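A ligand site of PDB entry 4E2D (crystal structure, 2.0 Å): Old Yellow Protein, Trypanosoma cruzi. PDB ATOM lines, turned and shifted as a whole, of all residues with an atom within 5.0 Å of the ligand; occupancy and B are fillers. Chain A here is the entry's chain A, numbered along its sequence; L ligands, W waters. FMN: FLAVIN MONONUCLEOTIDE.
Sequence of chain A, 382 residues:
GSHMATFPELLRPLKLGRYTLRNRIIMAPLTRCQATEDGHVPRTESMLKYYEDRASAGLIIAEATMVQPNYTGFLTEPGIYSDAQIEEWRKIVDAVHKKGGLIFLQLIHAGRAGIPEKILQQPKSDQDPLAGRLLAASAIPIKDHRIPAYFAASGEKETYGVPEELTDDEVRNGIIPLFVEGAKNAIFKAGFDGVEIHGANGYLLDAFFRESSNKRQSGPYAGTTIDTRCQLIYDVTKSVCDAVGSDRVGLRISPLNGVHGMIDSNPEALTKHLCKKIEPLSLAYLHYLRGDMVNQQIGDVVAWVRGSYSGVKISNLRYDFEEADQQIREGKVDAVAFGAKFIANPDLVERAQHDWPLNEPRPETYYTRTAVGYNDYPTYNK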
ATOM      1  N   ALA A  28     -17.000  12.421  -5.040  1.00  0.00           N
ATOM      2  CA  ALA A  28     -17.555  12.616  -6.388  1.00  0.00           C
ATOM      3  C   ALA A  28     -18.860  11.788  -6.637  1.00  0.00           C
ATOM      4  O   ALA A  28     -19.077  10.780  -5.988  1.00  0.00           O
ATOM      5  CB  ALA A  28     -16.526  12.314  -7.447  1.00  0.00           C
ATOM      6  N   PRO A  29     -19.731  12.265  -7.552  1.00  0.00           N
ATOM      7  CA  PRO A  29     -20.964  11.528  -7.860  1.00  0.00           C
ATOM      8  C   PRO A  29     -20.586  10.271  -8.656  1.00  0.00           C
ATOM      9  O   PRO A  29     -19.777  10.331  -9.584  1.00  0.00           O
ATOM     10  CB  PRO A  29     -21.749  12.511  -8.740  1.00  0.00           C
ATOM     11  CG  PRO A  29     -20.673  13.370  -9.360  1.00  0.00           C
ATOM     12  CD  PRO A  29     -19.734  13.595  -8.178  1.00  0.00           C
ATOM     13  N   LEU A  30     -21.165   9.153  -8.279  1.00  0.00           N
ATOM     14  CA  LEU A  30     -20.713   7.896  -8.809  1.00  0.00           C
ATOM     15  C   LEU A  30     -21.889   6.988  -8.996  1.00  0.00           C
ATOM     16  O   LEU A  30     -22.401   6.430  -8.025  1.00  0.00           O
ATOM     17  CB  LEU A  30     -19.661   7.258  -7.892  1.00  0.00           C
ATOM     18  CG  LEU A  30     -18.315   7.991  -7.801  1.00  0.00           C
ATOM     19  CD1 LEU A  30     -17.639   7.704  -6.434  1.00  0.00           C
ATOM     20  CD2 LEU A  30     -17.381   7.771  -9.002  1.00  0.00           C
ATOM     21  N   THR A  31     -22.280   6.836 -10.248  1.00  0.00           N
ATOM     22  CA  THR A  31     -23.287   5.877 -10.673  1.00  0.00           C
ATOM     23  C   THR A  31     -22.848   4.433 -10.436  1.00  0.00           C
ATOM     24  O   THR A  31     -21.831   3.979 -10.996  1.00  0.00           O
ATOM     25  CB  THR A  31     -23.534   6.032 -12.152  1.00  0.00           C
ATOM     26  OG1 THR A  31     -24.090   7.335 -12.376  1.00  0.00           O
ATOM     27  CG2 THR A  31     -24.514   4.928 -12.683  1.00  0.00           C
ATOM     28  N   ARG A  32     -23.622   3.706  -9.614  1.00  0.00           N
ATOM     29  CA  ARG A  32     -23.285   2.348  -9.238  1.00  0.00           C
ATOM     30  C   ARG A  32     -24.440   1.378  -9.545  1.00  0.00           C
ATOM     31  O   ARG A  32     -24.283   0.189  -9.336  1.00  0.00           O
ATOM     32  CB  ARG A  32     -22.914   2.241  -7.737  1.00  0.00           C
ATOM     33  CG  ARG A  32     -21.920   3.289  -7.224  1.00  0.00           C
ATOM     34  CD  ARG A  32     -20.612   3.249  -7.989  1.00  0.00           C
ATOM     35  NE  ARG A  32     -20.012   1.917  -8.056  1.00  0.00           N
ATOM     36  CZ  ARG A  32     -19.365   1.337  -7.051  1.00  0.00           C
ATOM     37  NH1 ARG A  32     -18.897   0.095  -7.209  1.00  0.00           N
ATOM     38  NH2 ARG A  32     -19.198   1.966  -5.912  1.00  0.00           N
ATOM     39  N   GLU A  63     -24.867   9.938  -6.464  1.00  0.00           N
ATOM     40  CA  GLU A  63     -24.907   9.586  -7.895  1.00  0.00           C
ATOM     41  C   GLU A  63     -26.012  10.267  -8.715  1.00  0.00           C
ATOM     42  O   GLU A  63     -27.072  10.616  -8.144  1.00  0.00           O
ATOM     43  CB  GLU A  63     -25.114   8.089  -7.994  1.00  0.00           C
ATOM     44  CG  GLU A  63     -26.357   7.575  -7.260  1.00  0.00           C
ATOM     45  CD  GLU A  63     -26.157   6.139  -6.817  1.00  0.00           C
ATOM     46  OE1 GLU A  63     -26.157   5.244  -7.703  1.00  0.00           O
ATOM     47  OE2 GLU A  63     -25.981   5.922  -5.595  1.00  0.00           O
ATOM     48  N   ALA A  64     -25.764  10.434 -10.020  1.00  0.00           N
ATOM     49  CA  ALA A  64     -26.760  10.960 -10.971  1.00  0.00           C
ATOM     50  C   ALA A  64     -28.101  10.280 -10.801  1.00  0.00           C
ATOM     51  O   ALA A  64     -28.189   9.064 -10.877  1.00  0.00           O
ATOM     52  CB  ALA A  64     -26.274  10.827 -12.425  1.00  0.00           C
ATOM     53  N   GLN A 106     -27.038  14.598  -6.943  1.00  0.00           N
ATOM     54  CA  GLN A 106     -26.849  15.070  -8.321  1.00  0.00           C
ATOM     55  C   GLN A 106     -28.118  14.734  -9.158  1.00  0.00           C
ATOM     56  O   GLN A 106     -28.635  13.639  -9.070  1.00  0.00           O
ATOM     57  CB  GLN A 106     -25.602  14.449  -8.958  1.00  0.00           C
ATOM     58  CG  GLN A 106     -25.264  15.088 -10.315  1.00  0.00           C
ATOM     59  CD  GLN A 106     -24.152  14.335 -11.017  1.00  0.00           C
ATOM     60  OE1 GLN A 106     -24.239  13.138 -11.201  1.00  0.00           O
ATOM     61  NE2 GLN A 106     -23.082  15.051 -11.395  1.00  0.00           N
ATOM     62  N   GLU A 196     -26.816  18.976  -6.892  1.00  0.00           N
ATOM     63  CA  GLU A 196     -25.789  19.353  -7.834  1.00  0.00           C
ATOM     64  C   GLU A 196     -26.439  19.223  -9.212  1.00  0.00           C
ATOM     65  O   GLU A 196     -26.934  18.185  -9.543  1.00  0.00           O
ATOM     66  CB  GLU A 196     -24.597  18.404  -7.755  1.00  0.00           C
ATOM     67  CG  GLU A 196     -23.512  18.817  -8.749  1.00  0.00           C
ATOM     68  CD  GLU A 196     -22.220  18.006  -8.633  1.00  0.00           C
ATOM     69  OE1 GLU A 196     -22.092  17.004  -9.395  1.00  0.00           O
ATOM     70  OE2 GLU A 196     -21.343  18.370  -7.797  1.00  0.00           O
ATOM     71  N   HIS A 198     -26.394  18.450 -13.038  1.00  0.00           N
ATOM     72  CA  HIS A 198     -25.457  17.670 -13.879  1.00  0.00           C
ATOM     73  C   HIS A 198     -25.262  18.310 -15.229  1.00  0.00           C
ATOM     74  O   HIS A 198     -25.909  17.974 -16.193  1.00  0.00           O
ATOM     75  CB  HIS A 198     -25.811  16.203 -13.930  1.00  0.00           C
ATOM     76  CG  HIS A 198     -24.688  15.320 -14.462  1.00  0.00           C
ATOM     77  ND1 HIS A 198     -23.678  15.790 -15.214  1.00  0.00           N
ATOM     78  CD2 HIS A 198     -24.459  13.970 -14.326  1.00  0.00           C
ATOM     79  CE1 HIS A 198     -22.857  14.808 -15.555  1.00  0.00           C
ATOM     80  NE2 HIS A 198     -23.295  13.703 -14.983  1.00  0.00           N
ATOM     81  N   ASN A 201     -20.292  15.664 -18.982  1.00  0.00           N
ATOM     82  CA  ASN A 201     -20.090  14.241 -19.323  1.00  0.00           C
ATOM     83  C   ASN A 201     -21.052  13.745 -20.434  1.00  0.00           C
ATOM     84  O   ASN A 201     -21.352  12.561 -20.546  1.00  0.00           O
ATOM     85  CB  ASN A 201     -20.154  13.334 -18.058  1.00  0.00           C
ATOM     86  CG  ASN A 201     -19.096  13.684 -17.027  1.00  0.00           C
ATOM     87  OD1 ASN A 201     -19.263  13.399 -15.834  1.00  0.00           O
ATOM     88  ND2 ASN A 201     -18.055  14.344 -17.447  1.00  0.00           N
ATOM     89  N   ARG A 252     -22.068  21.054 -11.807  1.00  0.00           N
ATOM     90  CA  ARG A 252     -20.913  20.339 -12.344  1.00  0.00           C
ATOM     91  C   ARG A 252     -20.813  20.504 -13.851  1.00  0.00           C
ATOM     92  O   ARG A 252     -21.823  20.362 -14.576  1.00  0.00           O
ATOM     93  CB  ARG A 252     -21.007  18.825 -12.053  1.00  0.00           C
ATOM     94  CG  ARG A 252     -19.652  18.162 -12.213  1.00  0.00           C
ATOM     95  CD  ARG A 252     -19.636  16.705 -11.816  1.00  0.00           C
ATOM     96  NE  ARG A 252     -18.310  16.322 -11.259  1.00  0.00           N
ATOM     97  CZ  ARG A 252     -17.844  15.062 -11.308  1.00  0.00           C
ATOM     98  NH1 ARG A 252     -16.668  14.721 -10.767  1.00  0.00           N
ATOM     99  NH2 ARG A 252     -18.574  14.149 -11.912  1.00  0.00           N
ATOM    100  N   LEU A 289     -14.621  18.870 -13.866  1.00  0.00           N
ATOM    101  CA  LEU A 289     -13.573  17.982 -14.266  1.00  0.00           C
ATOM    102  C   LEU A 289     -12.473  18.847 -14.873  1.00  0.00           C
ATOM    103  O   LEU A 289     -12.705  19.634 -15.821  1.00  0.00           O
ATOM    104  CB  LEU A 289     -14.071  16.911 -15.299  1.00  0.00           C
ATOM    105  CG  LEU A 289     -14.752  15.640 -14.773  1.00  0.00           C
ATOM    106  CD1 LEU A 289     -16.151  15.933 -14.197  1.00  0.00           C
ATOM    107  CD2 LEU A 289     -14.835  14.504 -15.833  1.00  0.00           C
ATOM    108  N   ASN A 316     -11.712  18.127  -9.883  1.00  0.00           N
ATOM    109  CA  ASN A 316     -11.727  16.684  -9.890  1.00  0.00           C
ATOM    110  C   ASN A 316     -10.956  16.174 -11.084  1.00  0.00           C
ATOM    111  O   ASN A 316     -10.911  16.869 -12.125  1.00  0.00           O
ATOM    112  CB  ASN A 316     -13.201  16.155  -9.965  1.00  0.00           C
ATOM    113  CG  ASN A 316     -13.256  14.691 -10.390  1.00  0.00           C
ATOM    114  OD1 ASN A 316     -13.171  13.779  -9.567  1.00  0.00           O
ATOM    115  ND2 ASN A 316     -13.361  14.465 -11.680  1.00  0.00           N
ATOM    116  N   LEU A 317     -10.357  14.994 -10.911  1.00  0.00           N
ATOM    117  CA  LEU A 317      -9.886  14.045 -11.968  1.00  0.00           C
ATOM    118  C   LEU A 317      -8.412  13.699 -11.745  1.00  0.00           C
ATOM    119  O   LEU A 317      -7.550  14.591 -11.922  1.00  0.00           O
ATOM    120  CB  LEU A 317     -10.083  14.591 -13.396  1.00  0.00           C
ATOM    121  CG  LEU A 317      -9.541  13.653 -14.515  1.00  0.00           C
ATOM    122  CD1 LEU A 317     -10.365  12.388 -14.567  1.00  0.00           C
ATOM    123  CD2 LEU A 317      -9.586  14.296 -15.892  1.00  0.00           C
ATOM    124  N   ARG A 318      -8.152  12.431 -11.364  1.00  0.00           N
ATOM    125  CA  ARG A 318      -6.809  11.893 -11.075  1.00  0.00           C
ATOM    126  C   ARG A 318      -6.003  12.733 -10.075  1.00  0.00           C
ATOM    127  O   ARG A 318      -4.789  12.962 -10.230  1.00  0.00           O
ATOM    128  CB  ARG A 318      -6.033  11.586 -12.366  1.00  0.00           C
ATOM    129  CG  ARG A 318      -6.807  10.698 -13.356  1.00  0.00           C
ATOM    130  CD  ARG A 318      -6.074  10.504 -14.685  1.00  0.00           C
ATOM    131  NE  ARG A 318      -5.979  11.777 -15.409  1.00  0.00           N
ATOM    132  CZ  ARG A 318      -6.597  12.043 -16.562  1.00  0.00           C
ATOM    133  NH1 ARG A 318      -7.363  11.142 -17.181  1.00  0.00           N
ATOM    134  NH2 ARG A 318      -6.464  13.229 -17.108  1.00  0.00           N
ATOM    135  N   TYR A 319      -6.683  13.191  -9.030  1.00  0.00           N
ATOM    136  CA  TYR A 319      -5.998  13.782  -7.891  1.00  0.00           C
ATOM    137  C   TYR A 319      -5.513  12.726  -6.882  1.00  0.00           C
ATOM    138  O   TYR A 319      -6.194  11.758  -6.654  1.00  0.00           O
ATOM    139  CB  TYR A 319      -6.918  14.769  -7.141  1.00  0.00           C
ATOM    140  CG  TYR A 319      -6.973  16.125  -7.806  1.00  0.00           C
ATOM    141  CD1 TYR A 319      -7.948  16.413  -8.754  1.00  0.00           C
ATOM    142  CD2 TYR A 319      -6.055  17.130  -7.455  1.00  0.00           C
ATOM    143  CE1 TYR A 319      -8.010  17.657  -9.349  1.00  0.00           C
ATOM    144  CE2 TYR A 319      -6.087  18.388  -8.082  1.00  0.00           C
ATOM    145  CZ  TYR A 319      -7.067  18.641  -9.035  1.00  0.00           C
ATOM    146  OH  TYR A 319      -7.178  19.908  -9.626  1.00  0.00           O
ATOM    147  N   ALA A 337     -12.830  16.777  -5.286  1.00  0.00           N
ATOM    148  CA  ALA A 337     -13.670  15.582  -5.296  1.00  0.00           C
ATOM    149  C   ALA A 337     -12.890  14.400  -5.834  1.00  0.00           C
ATOM    150  O   ALA A 337     -12.214  14.527  -6.824  1.00  0.00           O
ATOM    151  CB  ALA A 337     -14.917  15.812  -6.149  1.00  0.00           C
ATOM    152  N   PHE A 338     -13.040  13.243  -5.175  1.00  0.00           N
ATOM    153  CA  PHE A 338     -12.341  12.005  -5.544  1.00  0.00           C
ATOM    154  C   PHE A 338     -13.426  11.039  -5.925  1.00  0.00           C
ATOM    155  O   PHE A 338     -14.410  10.887  -5.181  1.00  0.00           O
ATOM    156  CB  PHE A 338     -11.582  11.453  -4.329  1.00  0.00           C
ATOM    157  CG  PHE A 338     -10.434  12.337  -3.901  1.00  0.00           C
ATOM    158  CD1 PHE A 338      -9.157  12.116  -4.388  1.00  0.00           C
ATOM    159  CD2 PHE A 338     -10.648  13.390  -3.015  1.00  0.00           C
ATOM    160  CE1 PHE A 338      -8.083  12.922  -3.999  1.00  0.00           C
ATOM    161  CE2 PHE A 338      -9.598  14.211  -2.634  1.00  0.00           C
ATOM    162  CZ  PHE A 338      -8.326  13.992  -3.130  1.00  0.00           C
ATOM    163  N   GLY A 339     -13.235  10.377  -7.061  1.00  0.00           N
ATOM    164  CA  GLY A 339     -14.128   9.309  -7.523  1.00  0.00           C
ATOM    165  C   GLY A 339     -13.670   7.905  -7.153  1.00  0.00           C
ATOM    166  O   GLY A 339     -14.124   7.373  -6.180  1.00  0.00           O
ATOM    167  N   ALA A 340     -12.763   7.332  -7.932  1.00  0.00           N
ATOM    168  CA  ALA A 340     -12.306   5.936  -7.737  1.00  0.00           C
ATOM    169  C   ALA A 340     -11.811   5.629  -6.294  1.00  0.00           C
ATOM    170  O   ALA A 340     -12.040   4.556  -5.763  1.00  0.00           O
ATOM    171  CB  ALA A 340     -11.237   5.592  -8.787  1.00  0.00           C
ATOM    172  N   ILE A 343     -14.682   5.021  -4.171  1.00  0.00           N
ATOM    173  CA  ILE A 343     -15.252   3.714  -4.442  1.00  0.00           C
ATOM    174  C   ILE A 343     -14.487   2.674  -3.618  1.00  0.00           C
ATOM    175  O   ILE A 343     -15.073   1.786  -3.030  1.00  0.00           O
ATOM    176  CB  ILE A 343     -15.116   3.332  -5.944  1.00  0.00           C
ATOM    177  CG1 ILE A 343     -16.076   4.160  -6.788  1.00  0.00           C
ATOM    178  CG2 ILE A 343     -15.371   1.854  -6.118  1.00  0.00           C
ATOM    179  CD1 ILE A 343     -15.698   4.087  -8.283  1.00  0.00           C
ATOM    180  N   TYR A 366     -17.186  -2.250 -10.858  1.00  0.00           N
ATOM    181  CA  TYR A 366     -17.859  -0.950 -10.556  1.00  0.00           C
ATOM    182  C   TYR A 366     -19.365  -1.043 -10.680  1.00  0.00           C
ATOM    183  O   TYR A 366     -20.088  -0.426  -9.885  1.00  0.00           O
ATOM    184  CB  TYR A 366     -17.387   0.204 -11.454  1.00  0.00           C
ATOM    185  CG  TYR A 366     -16.063   0.784 -11.116  1.00  0.00           C
ATOM    186  CD1 TYR A 366     -15.394   0.448  -9.932  1.00  0.00           C
ATOM    187  CD2 TYR A 366     -15.453   1.686 -12.012  1.00  0.00           C
ATOM    188  CE1 TYR A 366     -14.168   1.016  -9.620  1.00  0.00           C
ATOM    189  CE2 TYR A 366     -14.243   2.274 -11.711  1.00  0.00           C
ATOM    190  CZ  TYR A 366     -13.594   1.937 -10.518  1.00  0.00           C
ATOM    191  OH  TYR A 366     -12.367   2.490 -10.231  1.00  0.00           O
ATOM    192  N   TYR A 367     -19.823  -1.840 -11.646  1.00  0.00           N
ATOM    193  CA  TYR A 367     -21.255  -1.949 -11.938  1.00  0.00           C
ATOM    194  C   TYR A 367     -21.921  -3.328 -11.749  1.00  0.00           C
ATOM    195  O   TYR A 367     -22.819  -3.673 -12.539  1.00  0.00           O
ATOM    196  CB  TYR A 367     -21.510  -1.459 -13.385  1.00  0.00           C
ATOM    197  CG  TYR A 367     -20.911  -0.102 -13.748  1.00  0.00           C
ATOM    198  CD1 TYR A 367     -21.546   1.093 -13.372  1.00  0.00           C
ATOM    199  CD2 TYR A 367     -19.721  -0.025 -14.474  1.00  0.00           C
ATOM    200  CE1 TYR A 367     -21.007   2.334 -13.719  1.00  0.00           C
ATOM    201  CE2 TYR A 367     -19.157   1.222 -14.810  1.00  0.00           C
ATOM    202  CZ  TYR A 367     -19.812   2.387 -14.440  1.00  0.00           C
ATOM    203  OH  TYR A 367     -19.253   3.607 -14.801  1.00  0.00           O
HETATM  204  N1  FMN L   1     -19.746  11.718 -12.782  1.00  0.00           N
HETATM  205  C2  FMN L   1     -20.939  12.327 -12.591  1.00  0.00           C
HETATM  206  O2  FMN L   1     -20.929  13.579 -12.728  1.00  0.00           O
HETATM  207  N3  FMN L   1     -22.073  11.628 -12.304  1.00  0.00           N
HETATM  208  C4  FMN L   1     -22.056  10.307 -12.136  1.00  0.00           C
HETATM  209  O4  FMN L   1     -23.072   9.629 -11.819  1.00  0.00           O
HETATM  210  C4A FMN L   1     -20.784   9.582 -12.294  1.00  0.00           C
HETATM  211  N5  FMN L   1     -20.697   8.232 -12.151  1.00  0.00           N
HETATM  212  C5A FMN L   1     -19.515   7.563 -12.260  1.00  0.00           C
HETATM  213  C6  FMN L   1     -19.479   6.174 -12.046  1.00  0.00           C
HETATM  214  C7  FMN L   1     -18.275   5.513 -12.151  1.00  0.00           C
HETATM  215  C7M FMN L   1     -18.278   4.025 -11.939  1.00  0.00           C
HETATM  216  C8  FMN L   1     -17.030   6.245 -12.481  1.00  0.00           C
HETATM  217  C8M FMN L   1     -15.689   5.524 -12.568  1.00  0.00           C
HETATM  218  C9  FMN L   1     -17.046   7.625 -12.649  1.00  0.00           C
HETATM  219  C9A FMN L   1     -18.274   8.316 -12.528  1.00  0.00           C
HETATM  220  N10 FMN L   1     -18.379   9.719 -12.742  1.00  0.00           N
HETATM  221  C10 FMN L   1     -19.611  10.366 -12.605  1.00  0.00           C
HETATM  222  C1' FMN L   1     -17.214  10.584 -12.967  1.00  0.00           C
HETATM  223  C2' FMN L   1     -16.658  10.755 -11.507  1.00  0.00           C
HETATM  224  O2' FMN L   1     -17.545  11.581 -10.724  1.00  0.00           O
HETATM  225  C3' FMN L   1     -15.236  11.340 -11.487  1.00  0.00           C
HETATM  226  O3' FMN L   1     -15.329  12.619 -12.150  1.00  0.00           O
HETATM  227  C4' FMN L   1     -14.253  10.423 -12.252  1.00  0.00           C
HETATM  228  O4' FMN L   1     -14.128   9.155 -11.579  1.00  0.00           O
HETATM  229  C5' FMN L   1     -12.847  10.987 -12.318  1.00  0.00           C
HETATM  230  O5' FMN L   1     -12.470  11.152 -10.936  1.00  0.00           O
HETATM  231  P   FMN L   1     -11.321  10.250 -10.276  1.00  0.00           P
HETATM  232  O1P FMN L   1     -10.095  10.389 -11.150  1.00  0.00           O
HETATM  233  O2P FMN L   1     -11.917   8.881 -10.149  1.00  0.00           O
HETATM  234  O3P FMN L   1     -11.088  10.810  -8.912  1.00  0.00           O
HETATM  235  O   HOH W   1     -10.002   8.892 -13.626  1.00  0.00           O
HETATM  236  O   HOH W   2     -18.652  10.362 -15.746  1.00  0.00           O
HETATM  237  O   HOH W   3     -21.449  11.023 -15.565  1.00  0.00           O
HETATM  238  O   HOH W   4      -8.010   8.753 -10.249  1.00  0.00           O
HETATM  239  O   HOH W   5      -9.990   9.309  -7.014  1.00  0.00           O
HETATM  240  O   HOH W   6      -9.903  13.375  -8.610  1.00  0.00           O
HETATM  241  O   HOH W   7     -11.760   6.988 -12.073  1.00  0.00           O
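An oxygen (O2') of the ligand is in hydrogen-bond range of the backbone carbonyl oxygen of Pro 29 (2.8 Å).
The side-chain hydroxyl (OG1) of Thr 31 is in hydrogen-bond range of an oxygen (O4) of the ligand (2.6 Å).
The guanidinium group of Arg 252 lies within hydrogen-bond range of an oxygen (O2) of the ligand (2.6 Å).
O3' of the ligand lies within hydrogen-bond range of ND2 of Asn 316 (2.7 Å).
N of Ala 64 lies within hydrogen-bond range of O4 of the ligand (3.3 Å).
A nitrogen (N5) of the ligand sits at hydrogen-bond distance from the backbone NH (N) of Thr 31 (2.8 Å).
An oxygen (O3P) of the ligand is in hydrogen-bond range of the backbone NH (N) of Gly 339 (2.9 Å).
An oxygen (O2) of the ligand sits at hydrogen-bond distance from a ring nitrogen (NE2) of His 198 (3.3 Å).
The side-chain amide oxygen (OE1) of Gln 106 sits at hydrogen-bond distance from a nitrogen (N3) of the ligand, at 2.9 Å.
An oxygen (O1P) of the ligand lies within hydrogen-bond range of the backbone NH (N) of Arg 318, at 2.8 Å.
N of Ala 340 lies within hydrogen-bond range of O2P of the ligand, at 2.8 Å.
The side-chain amide nitrogen (ND2) of Asn 316 lies close to the guanidinium group (NH1) of Arg 252, 3.4 Å away.
N of Ala 28 lies within hydrogen-bond range of O of Phe 338 (3.0 Å).
The side-chain amide oxygen (OE1) of Gln 106 sits close to the backbone NH (N) of Ala 64.
O of Tyr 366 is in hydrogen-bond range of NE of Arg 32 (3.0 Å).
The backbone carbonyl oxygen (O) of Ala 337 lies close to the side-chain amide oxygen (OD1) of Asn 316 (3.0 Å).
The side-chain amide nitrogen (NE2) of Gln 106 sits at hydrogen-bond distance from the side-chain carboxylate (OE1) of Glu 196 (3.0 Å).
Merely in contact with the ligand: Ala 28 (3.5 Å), Leu 30 (3.4 Å), Asn 201 (3.5 Å), Leu 289 (3.98 Å), Leu 317 (3.6 Å), Phe 338 (3.8 Å), Tyr 366 (3.7 Å) and Tyr 367 (3.1 Å).
Hydrophobic or aromatic side chains that line the ligand: Ala 28, Pro 29, Leu 30, Ala 64, His 198, Leu 289, Leu 317, Ala 340, Tyr 366 and Tyr 367.
The nearest printed residue that does not touch the ligand is Glu 63 (4.3 Å).
Water W5 lies within hydrogen-bond range of O3P of the ligand (2.7 Å) and N of Gly 339 (3.4 Å).
Water W2 lies within hydrogen-bond range of the side-chain amide oxygen (OD1) of Asn 201 and a nitrogen (N1) of the ligand.
Water W3 lies within hydrogen-bond range of OD1 of Asn 201, NE2 of His 198 and N1 of the ligand.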
